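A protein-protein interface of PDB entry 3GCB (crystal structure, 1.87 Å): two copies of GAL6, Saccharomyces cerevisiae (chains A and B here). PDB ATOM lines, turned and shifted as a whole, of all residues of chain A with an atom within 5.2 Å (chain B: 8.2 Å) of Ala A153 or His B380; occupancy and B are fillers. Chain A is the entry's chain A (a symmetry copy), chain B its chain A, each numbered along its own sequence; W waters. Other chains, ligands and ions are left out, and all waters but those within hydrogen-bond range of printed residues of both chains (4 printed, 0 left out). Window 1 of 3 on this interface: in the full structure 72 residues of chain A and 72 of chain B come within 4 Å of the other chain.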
ATOM      1  N   GLN A 149      -0.013  -2.348  16.788  1.00  0.00           N
ATOM      2  CA  GLN A 149       1.181  -2.953  16.200  1.00  0.00           C
ATOM      3  C   GLN A 149       1.046  -3.101  14.687  1.00  0.00           C
ATOM      4  O   GLN A 149       2.020  -2.943  13.936  1.00  0.00           O
ATOM      5  CB  GLN A 149       1.493  -4.294  16.870  1.00  0.00           C
ATOM      6  CG  GLN A 149       2.147  -4.113  18.255  1.00  0.00           C
ATOM      7  CD  GLN A 149       3.463  -3.332  18.184  1.00  0.00           C
ATOM      8  OE1 GLN A 149       4.380  -3.708  17.453  1.00  0.00           O
ATOM      9  NE2 GLN A 149       3.546  -2.233  18.913  1.00  0.00           N
ATOM     10  N   TYR A 150      -0.158  -3.420  14.233  1.00  0.00           N
ATOM     11  CA  TYR A 150      -0.395  -3.543  12.805  1.00  0.00           C
ATOM     12  C   TYR A 150      -0.248  -2.166  12.125  1.00  0.00           C
ATOM     13  O   TYR A 150       0.299  -2.074  11.021  1.00  0.00           O
ATOM     14  CB  TYR A 150      -1.790  -4.102  12.512  1.00  0.00           C
ATOM     15  CG  TYR A 150      -1.997  -4.341  11.028  1.00  0.00           C
ATOM     16  CD1 TYR A 150      -1.446  -5.458  10.411  1.00  0.00           C
ATOM     17  CD2 TYR A 150      -2.663  -3.409  10.230  1.00  0.00           C
ATOM     18  CE1 TYR A 150      -1.537  -5.641   9.055  1.00  0.00           C
ATOM     19  CE2 TYR A 150      -2.763  -3.583   8.854  1.00  0.00           C
ATOM     20  CZ  TYR A 150      -2.191  -4.700   8.271  1.00  0.00           C
ATOM     21  OH  TYR A 150      -2.226  -4.855   6.913  1.00  0.00           O
ATOM     22  N   LEU A 151      -0.758  -1.103  12.759  1.00  0.00           N
ATOM     23  CA  LEU A 151      -0.653   0.246  12.182  1.00  0.00           C
ATOM     24  C   LEU A 151       0.809   0.667  12.002  1.00  0.00           C
ATOM     25  O   LEU A 151       1.160   1.326  11.019  1.00  0.00           O
ATOM     26  CB  LEU A 151      -1.371   1.280  13.061  1.00  0.00           C
ATOM     27  CG  LEU A 151      -2.902   1.196  13.107  1.00  0.00           C
ATOM     28  CD1 LEU A 151      -3.467   2.098  14.197  1.00  0.00           C
ATOM     29  CD2 LEU A 151      -3.487   1.551  11.723  1.00  0.00           C
ATOM     30  N   LEU A 152       1.646   0.276  12.963  1.00  0.00           N
ATOM     31  CA  LEU A 152       3.066   0.613  12.975  1.00  0.00           C
ATOM     32  C   LEU A 152       3.945  -0.224  12.058  1.00  0.00           C
ATOM     33  O   LEU A 152       5.096   0.130  11.817  1.00  0.00           O
ATOM     34  CB  LEU A 152       3.600   0.470  14.398  1.00  0.00           C
ATOM     35  CG  LEU A 152       3.031   1.403  15.475  1.00  0.00           C
ATOM     36  CD1 LEU A 152       3.460   0.911  16.854  1.00  0.00           C
ATOM     37  CD2 LEU A 152       3.551   2.826  15.236  1.00  0.00           C
ATOM     38  N   ALA A 153       3.414  -1.336  11.564  1.00  0.00           N
ATOM     39  CA  ALA A 153       4.195  -2.242  10.720  1.00  0.00           C
ATOM     40  C   ALA A 153       4.566  -1.693   9.351  1.00  0.00           C
ATOM     41  O   ALA A 153       5.725  -1.737   9.000  1.00  0.00           O
ATOM     42  CB  ALA A 153       3.495  -3.569  10.576  1.00  0.00           C
ATOM     43  N   ALA A 154       3.606  -1.177   8.584  1.00  0.00           N
ATOM     44  CA  ALA A 154       3.920  -0.664   7.245  1.00  0.00           C
ATOM     45  C   ALA A 154       3.020   0.509   6.841  1.00  0.00           C
ATOM     46  O   ALA A 154       2.368   0.468   5.795  1.00  0.00           O
ATOM     47  CB  ALA A 154       3.804  -1.794   6.222  1.00  0.00           C
ATOM     48  N   PRO A 155       3.071   1.614   7.603  1.00  0.00           N
ATOM     49  CA  PRO A 155       2.236   2.786   7.318  1.00  0.00           C
ATOM     50  C   PRO A 155       2.355   3.421   5.938  1.00  0.00           C
ATOM     51  O   PRO A 155       1.389   4.007   5.448  1.00  0.00           O
ATOM     52  CB  PRO A 155       2.621   3.767   8.439  1.00  0.00           C
ATOM     53  CG  PRO A 155       4.055   3.387   8.776  1.00  0.00           C
ATOM     54  CD  PRO A 155       3.999   1.873   8.733  1.00  0.00           C
ATOM     55  N   THR A 198       8.892   5.850   7.454  1.00  0.00           N
ATOM     56  CA  THR A 198       8.326   4.991   8.470  1.00  0.00           C
ATOM     57  C   THR A 198       9.011   5.119   9.810  1.00  0.00           C
ATOM     58  O   THR A 198       8.356   5.084  10.842  1.00  0.00           O
ATOM     59  CB  THR A 198       8.266   3.557   7.949  1.00  0.00           C
ATOM     60  OG1 THR A 198       7.428   3.542   6.782  1.00  0.00           O
ATOM     61  CG2 THR A 198       7.679   2.630   8.984  1.00  0.00           C
ATOM     62  N   ARG A 202       6.990   6.371  13.129  1.00  0.00           N
ATOM     63  CA  ARG A 202       6.982   5.583  14.369  1.00  0.00           C
ATOM     64  C   ARG A 202       7.370   6.468  15.562  1.00  0.00           C
ATOM     65  O   ARG A 202       6.896   6.278  16.697  1.00  0.00           O
ATOM     66  CB  ARG A 202       7.890   4.355  14.230  1.00  0.00           C
ATOM     67  CG  ARG A 202       7.304   3.322  13.273  1.00  0.00           C
ATOM     68  CD  ARG A 202       8.300   2.217  13.026  1.00  0.00           C
ATOM     69  NE  ARG A 202       7.731   1.194  12.156  1.00  0.00           N
ATOM     70  CZ  ARG A 202       8.451   0.459  11.308  1.00  0.00           C
ATOM     71  NH1 ARG A 202       9.768   0.643  11.207  1.00  0.00           N
ATOM     72  NH2 ARG A 202       7.861  -0.489  10.597  1.00  0.00           N
ATOM     73  N   HIS B 343      20.213  -5.695  15.226  1.00  0.00           N
ATOM     74  CA  HIS B 343      19.316  -5.264  14.189  1.00  0.00           C
ATOM     75  C   HIS B 343      20.060  -5.003  12.873  1.00  0.00           C
ATOM     76  O   HIS B 343      20.389  -3.859  12.544  1.00  0.00           O
ATOM     77  CB  HIS B 343      18.538  -4.008  14.615  1.00  0.00           C
ATOM     78  CG  HIS B 343      17.412  -3.670  13.690  1.00  0.00           C
ATOM     79  ND1 HIS B 343      16.474  -2.699  13.973  1.00  0.00           N
ATOM     80  CD2 HIS B 343      17.083  -4.155  12.467  1.00  0.00           C
ATOM     81  CE1 HIS B 343      15.628  -2.600  12.966  1.00  0.00           C
ATOM     82  NE2 HIS B 343      15.977  -3.471  12.039  1.00  0.00           N
ATOM     83  N   LYS B 346      20.583  -2.236  10.004  1.00  0.00           N
ATOM     84  CA  LYS B 346      20.491  -0.834  10.417  1.00  0.00           C
ATOM     85  C   LYS B 346      21.899  -0.257  10.583  1.00  0.00           C
ATOM     86  O   LYS B 346      22.764  -0.848  11.237  1.00  0.00           O
ATOM     87  CB  LYS B 346      19.738  -0.709  11.743  1.00  0.00           C
ATOM     88  CG  LYS B 346      18.252  -0.774  11.615  1.00  0.00           C
ATOM     89  CD  LYS B 346      17.708   0.529  11.072  1.00  0.00           C
ATOM     90  CE  LYS B 346      16.204   0.411  10.934  1.00  0.00           C
ATOM     91  NZ  LYS B 346      15.587   1.622  10.318  1.00  0.00           N
ATOM     92  N   GLN B 371      13.900   9.190  18.917  1.00  0.00           N
ATOM     93  CA  GLN B 371      13.290   8.018  19.591  1.00  0.00           C
ATOM     94  C   GLN B 371      14.325   7.108  20.240  1.00  0.00           C
ATOM     95  O   GLN B 371      15.274   6.646  19.601  1.00  0.00           O
ATOM     96  CB  GLN B 371      12.375   7.241  18.652  1.00  0.00           C
ATOM     97  CG  GLN B 371      11.401   6.293  19.363  1.00  0.00           C
ATOM     98  CD  GLN B 371      10.339   5.732  18.410  1.00  0.00           C
ATOM     99  OE1 GLN B 371      10.663   5.226  17.345  1.00  0.00           O
ATOM    100  NE2 GLN B 371       9.068   5.805  18.807  1.00  0.00           N
ATOM    101  N   ALA B 374      14.297   1.795  24.001  1.00  0.00           N
ATOM    102  CA  ALA B 374      13.126   1.082  24.494  1.00  0.00           C
ATOM    103  C   ALA B 374      11.929   1.389  23.618  1.00  0.00           C
ATOM    104  O   ALA B 374      11.186   0.479  23.266  1.00  0.00           O
ATOM    105  CB  ALA B 374      12.837   1.470  25.937  1.00  0.00           C
ATOM    106  N   SER B 375      11.761   2.665  23.254  1.00  0.00           N
ATOM    107  CA  SER B 375      10.647   3.089  22.400  1.00  0.00           C
ATOM    108  C   SER B 375      10.767   2.572  20.965  1.00  0.00           C
ATOM    109  O   SER B 375       9.754   2.255  20.349  1.00  0.00           O
ATOM    110  CB  SER B 375      10.490   4.602  22.399  1.00  0.00           C
ATOM    111  OG  SER B 375      10.191   5.070  23.700  1.00  0.00           O
ATOM    112  N   ARG B 376      11.985   2.488  20.428  1.00  0.00           N
ATOM    113  CA  ARG B 376      12.159   1.944  19.074  1.00  0.00           C
ATOM    114  C   ARG B 376      11.657   0.496  19.065  1.00  0.00           C
ATOM    115  O   ARG B 376      11.008   0.063  18.123  1.00  0.00           O
ATOM    116  CB  ARG B 376      13.620   1.977  18.641  1.00  0.00           C
ATOM    117  CG  ARG B 376      14.148   3.372  18.423  1.00  0.00           C
ATOM    118  CD  ARG B 376      15.466   3.307  17.693  1.00  0.00           C
ATOM    119  NE  ARG B 376      16.551   2.648  18.425  1.00  0.00           N
ATOM    120  CZ  ARG B 376      17.426   3.277  19.216  1.00  0.00           C
ATOM    121  NH1 ARG B 376      17.333   4.588  19.426  1.00  0.00           N
ATOM    122  NH2 ARG B 376      18.484   2.616  19.676  1.00  0.00           N
ATOM    123  N   ILE B 377      11.942  -0.244  20.132  1.00  0.00           N
ATOM    124  CA  ILE B 377      11.483  -1.621  20.226  1.00  0.00           C
ATOM    125  C   ILE B 377       9.965  -1.682  20.347  1.00  0.00           C
ATOM    126  O   ILE B 377       9.320  -2.436  19.628  1.00  0.00           O
ATOM    127  CB  ILE B 377      12.118  -2.343  21.423  1.00  0.00           C
ATOM    128  CG1 ILE B 377      13.646  -2.248  21.345  1.00  0.00           C
ATOM    129  CG2 ILE B 377      11.681  -3.799  21.435  1.00  0.00           C
ATOM    130  CD1 ILE B 377      14.361  -2.805  22.590  1.00  0.00           C
ATOM    131  N   ARG B 378       9.393  -0.888  21.257  1.00  0.00           N
ATOM    132  CA  ARG B 378       7.943  -0.867  21.451  1.00  0.00           C
ATOM    133  C   ARG B 378       7.146  -0.429  20.235  1.00  0.00           C
ATOM    134  O   ARG B 378       6.056  -0.943  19.973  1.00  0.00           O
ATOM    135  CB  ARG B 378       7.576   0.060  22.610  1.00  0.00           C
ATOM    136  CG  ARG B 378       7.995  -0.491  23.952  1.00  0.00           C
ATOM    137  CD  ARG B 378       7.290   0.226  25.098  1.00  0.00           C
ATOM    138  NE  ARG B 378       7.509  -0.456  26.380  1.00  0.00           N
ATOM    139  CZ  ARG B 378       8.392  -0.068  27.300  1.00  0.00           C
ATOM    140  NH1 ARG B 378       9.159   1.001  27.090  1.00  0.00           N
ATOM    141  NH2 ARG B 378       8.461  -0.714  28.466  1.00  0.00           N
ATOM    142  N   TYR B 379       7.689   0.546  19.514  1.00  0.00           N
ATOM    143  CA  TYR B 379       7.036   1.131  18.350  1.00  0.00           C
ATOM    144  C   TYR B 379       7.298   0.483  17.002  1.00  0.00           C
ATOM    145  O   TYR B 379       7.051   1.089  15.955  1.00  0.00           O
ATOM    146  CB  TYR B 379       7.285   2.653  18.317  1.00  0.00           C
ATOM    147  CG  TYR B 379       6.358   3.365  19.274  1.00  0.00           C
ATOM    148  CD1 TYR B 379       6.590   3.348  20.663  1.00  0.00           C
ATOM    149  CD2 TYR B 379       5.174   3.940  18.809  1.00  0.00           C
ATOM    150  CE1 TYR B 379       5.637   3.885  21.569  1.00  0.00           C
ATOM    151  CE2 TYR B 379       4.225   4.470  19.693  1.00  0.00           C
ATOM    152  CZ  TYR B 379       4.458   4.438  21.060  1.00  0.00           C
ATOM    153  OH  TYR B 379       3.490   4.951  21.895  1.00  0.00           O
ATOM    154  N   HIS B 380       7.776  -0.757  17.035  1.00  0.00           N
ATOM    155  CA  HIS B 380       7.990  -1.534  15.813  1.00  0.00           C
ATOM    156  C   HIS B 380       9.126  -1.046  14.928  1.00  0.00           C
ATOM    157  O   HIS B 380       9.209  -1.429  13.772  1.00  0.00           O
ATOM    158  CB  HIS B 380       6.681  -1.568  15.016  1.00  0.00           C
ATOM    159  CG  HIS B 380       6.525  -2.774  14.153  1.00  0.00           C
ATOM    160  ND1 HIS B 380       5.423  -3.590  14.213  1.00  0.00           N
ATOM    161  CD2 HIS B 380       7.343  -3.304  13.225  1.00  0.00           C
ATOM    162  CE1 HIS B 380       5.567  -4.590  13.358  1.00  0.00           C
ATOM    163  NE2 HIS B 380       6.735  -4.438  12.744  1.00  0.00           N
ATOM    164  N   GLU B 381      10.042  -0.259  15.486  1.00  0.00           N
ATOM    165  CA  GLU B 381      11.156   0.276  14.698  1.00  0.00           C
ATOM    166  C   GLU B 381      12.441  -0.556  14.752  1.00  0.00           C
ATOM    167  O   GLU B 381      13.183  -0.629  13.770  1.00  0.00           O
ATOM    168  CB  GLU B 381      11.443   1.723  15.127  1.00  0.00           C
ATOM    169  CG  GLU B 381      12.733   2.306  14.541  1.00  0.00           C
ATOM    170  CD  GLU B 381      12.722   2.442  13.011  1.00  0.00           C
ATOM    171  OE1 GLU B 381      11.637   2.409  12.389  1.00  0.00           O
ATOM    172  OE2 GLU B 381      13.818   2.602  12.436  1.00  0.00           O
ATOM    173  N   SER B 382      12.729  -1.153  15.900  1.00  0.00           N
ATOM    174  CA  SER B 382      13.945  -1.937  16.017  1.00  0.00           C
ATOM    175  C   SER B 382      13.684  -3.275  16.711  1.00  0.00           C
ATOM    176  O   SER B 382      12.860  -3.360  17.608  1.00  0.00           O
ATOM    177  CB  SER B 382      15.027  -1.131  16.753  1.00  0.00           C
ATOM    178  OG  SER B 382      16.318  -1.664  16.468  1.00  0.00           O
ATOM    179  N   LEU B 383      14.380  -4.311  16.243  1.00  0.00           N
ATOM    180  CA  LEU B 383      14.254  -5.679  16.756  1.00  0.00           C
ATOM    181  C   LEU B 383      15.535  -6.452  16.421  1.00  0.00           C
ATOM    182  O   LEU B 383      16.410  -5.953  15.691  1.00  0.00           O
ATOM    183  CB  LEU B 383      13.070  -6.387  16.075  1.00  0.00           C
ATOM    184  CG  LEU B 383      13.250  -6.860  14.617  1.00  0.00           C
ATOM    185  CD1 LEU B 383      12.104  -7.751  14.198  1.00  0.00           C
ATOM    186  CD2 LEU B 383      13.380  -5.684  13.641  1.00  0.00           C
ATOM    187  N   TRP B 463       5.690 -13.487  19.450  1.00  0.00           N
ATOM    188  CA  TRP B 463       6.052 -12.540  18.384  1.00  0.00           C
ATOM    189  C   TRP B 463       6.900 -11.359  18.838  1.00  0.00           C
ATOM    190  O   TRP B 463       7.045 -10.394  18.088  1.00  0.00           O
ATOM    191  CB  TRP B 463       4.806 -12.006  17.684  1.00  0.00           C
ATOM    192  CG  TRP B 463       3.841 -11.419  18.629  1.00  0.00           C
ATOM    193  CD1 TRP B 463       3.970 -10.251  19.332  1.00  0.00           C
ATOM    194  CD2 TRP B 463       2.597 -11.998  19.017  1.00  0.00           C
ATOM    195  NE1 TRP B 463       2.882 -10.081  20.144  1.00  0.00           N
ATOM    196  CE2 TRP B 463       2.028 -11.137  19.978  1.00  0.00           C
ATOM    197  CE3 TRP B 463       1.913 -13.169  18.659  1.00  0.00           C
ATOM    198  CZ2 TRP B 463       0.805 -11.409  20.581  1.00  0.00           C
ATOM    199  CZ3 TRP B 463       0.708 -13.443  19.250  1.00  0.00           C
ATOM    200  CH2 TRP B 463       0.161 -12.564  20.210  1.00  0.00           C
ATOM    201  N   PRO B 465       9.815  -8.671  19.572  1.00  0.00           N
ATOM    202  CA  PRO B 465      10.968  -8.271  18.762  1.00  0.00           C
ATOM    203  C   PRO B 465      12.295  -8.845  19.237  1.00  0.00           C
ATOM    204  O   PRO B 465      13.256  -8.933  18.464  1.00  0.00           O
ATOM    205  CB  PRO B 465      10.932  -6.727  18.816  1.00  0.00           C
ATOM    206  CG  PRO B 465       9.974  -6.405  19.923  1.00  0.00           C
ATOM    207  CD  PRO B 465       8.963  -7.512  19.870  1.00  0.00           C
HETATM  208  O   HOH W   1       7.264  -3.908  18.252  1.00  0.00           O
HETATM  209  O   HOH W   2      11.754   2.041   9.009  1.00  0.00           O
HETATM  210  O   HOH W   3       6.618  -4.687   9.660  1.00  0.00           O
HETATM  211  O   HOH W   4       4.989  -3.053  21.933  1.00  0.00           O
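No position is printed for both chains. Of the 9 pairs that touch across the chains among the printed residues, none has its exchanged pair printed and touching as well.
Printed residues of chain B within 4 Å of Leu A152: Tyr B379 and His B380. Printed residues of chain A within 4 Å of Gln B371: Arg A202. Printed residues of chain A within 4 Å of Arg B378: Gln A149. Of the printed residues of chain A, Tyr B379 touches Leu A152 (3.7 Å) and Arg A202 (3.4 Å). Of chain A, only Gln A149 (3.4 Å), Leu A152 (3.7 Å), Ala A153 (3.6 Å) and Arg A202 (3.2 Å) come within 4 Å of His B380. The nearest residue of chain B that does not touch Ala A153 is Tyr B379 (6.2 Å). The nearest printed residue of chain A that does not touch His B380 is Tyr A150 (5.6 Å). The nearest printed residue of chain B that does not touch Gln A149 is Tyr B379 (4.9 Å).
O of Arg A202 lies within hydrogen-bond range of NE2 of Gln B371 (3.1 Å). O of Arg B378 is in hydrogen-bond range of NE2 of Gln A149. A ring nitrogen (ND1) of His B380 is in hydrogen-bond range of the side-chain amide oxygen (OE1) of Gln A149 (3.4 Å). The backbone carbonyl oxygen (O) of His B380 lies close to the guanidinium group (NH1) of Arg A202, at 3.3 Å. The guanidinium group (NH1) of Arg A202 lies within salt-bridge range of the side-chain carboxylate (OE1) of Glu B381, 2.8 Å away.
Of the 15 printed residues of chain B, 5 touch a printed residue of chain A. Printed residues of chain B that touch a printed residue of chain A: Gln B371, Arg B378, Tyr B379, His B380 and Glu B381. Hydrophobic or aromatic side chains of chain B within 4 Å of the printed part of chain A: Tyr B379 and His B380. Of the 9 printed residues of chain A, 4 touch a printed residue of chain B. Hydrophobic or aromatic side chains of chain A within 4 Å of the printed part of chain B: Leu A152 and Ala A153. Along chain A the printed residues that touch a printed residue of chain B span positions 149 to 202. Among the printed residues, 9 pairs touch across the chains. Among the printed residues, Asp or Glu carboxylates within 4 Å of a Lys or Arg side-chain nitrogen of the other chain: Arg A202 with Glu B381.
Water W1 lies within hydrogen-bond range of O of Ile B377 (2.9 Å), OE1 of Gln A149 (3.0 Å) and N of His B380 (3.4 Å). Water W4 lies within hydrogen-bond range of O of Arg B378 (3.1 Å) and NE2 of Gln A149 (3.4 Å). Water W3 lies within hydrogen-bond range of a ring nitrogen (NE2) of His B380 and the backbone carbonyl oxygen of Ala A153. Water W2 lies within hydrogen-bond range of NH1 of Arg A202 (3.3 Å) and OE1 of Glu B381 (3.4 Å).
Leu A152 touches Tyr B379 (CD1 to O, 3.7 Å). Leu A152 touches His B380. CB of Ala A153 touches CE1 of His B380, at 3.6 Å. CD of Arg A202 touches O of Tyr B379 (3.4 Å).
NZ of Lys B346 is in salt-bridge range of OE2 of Glu B381 (2.9 Å). The guanidinium group (NH1) of Arg B376 lies within hydrogen-bond range of the backbone carbonyl oxygen (O) of Gln B371 (2.9 Å). The backbone NH (N) of Glu B381 sits at hydrogen-bond distance from the backbone carbonyl oxygen (O) of Arg B376, 2.8 Å away. The guanidinium group (NE) of Arg A202 is in hydrogen-bond range of the backbone carbonyl oxygen (O) of Leu A152 (2.9 Å). The backbone carbonyl oxygen (O) of Ala A153 lies within hydrogen-bond range of the guanidinium group (NH2) of Arg A202.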
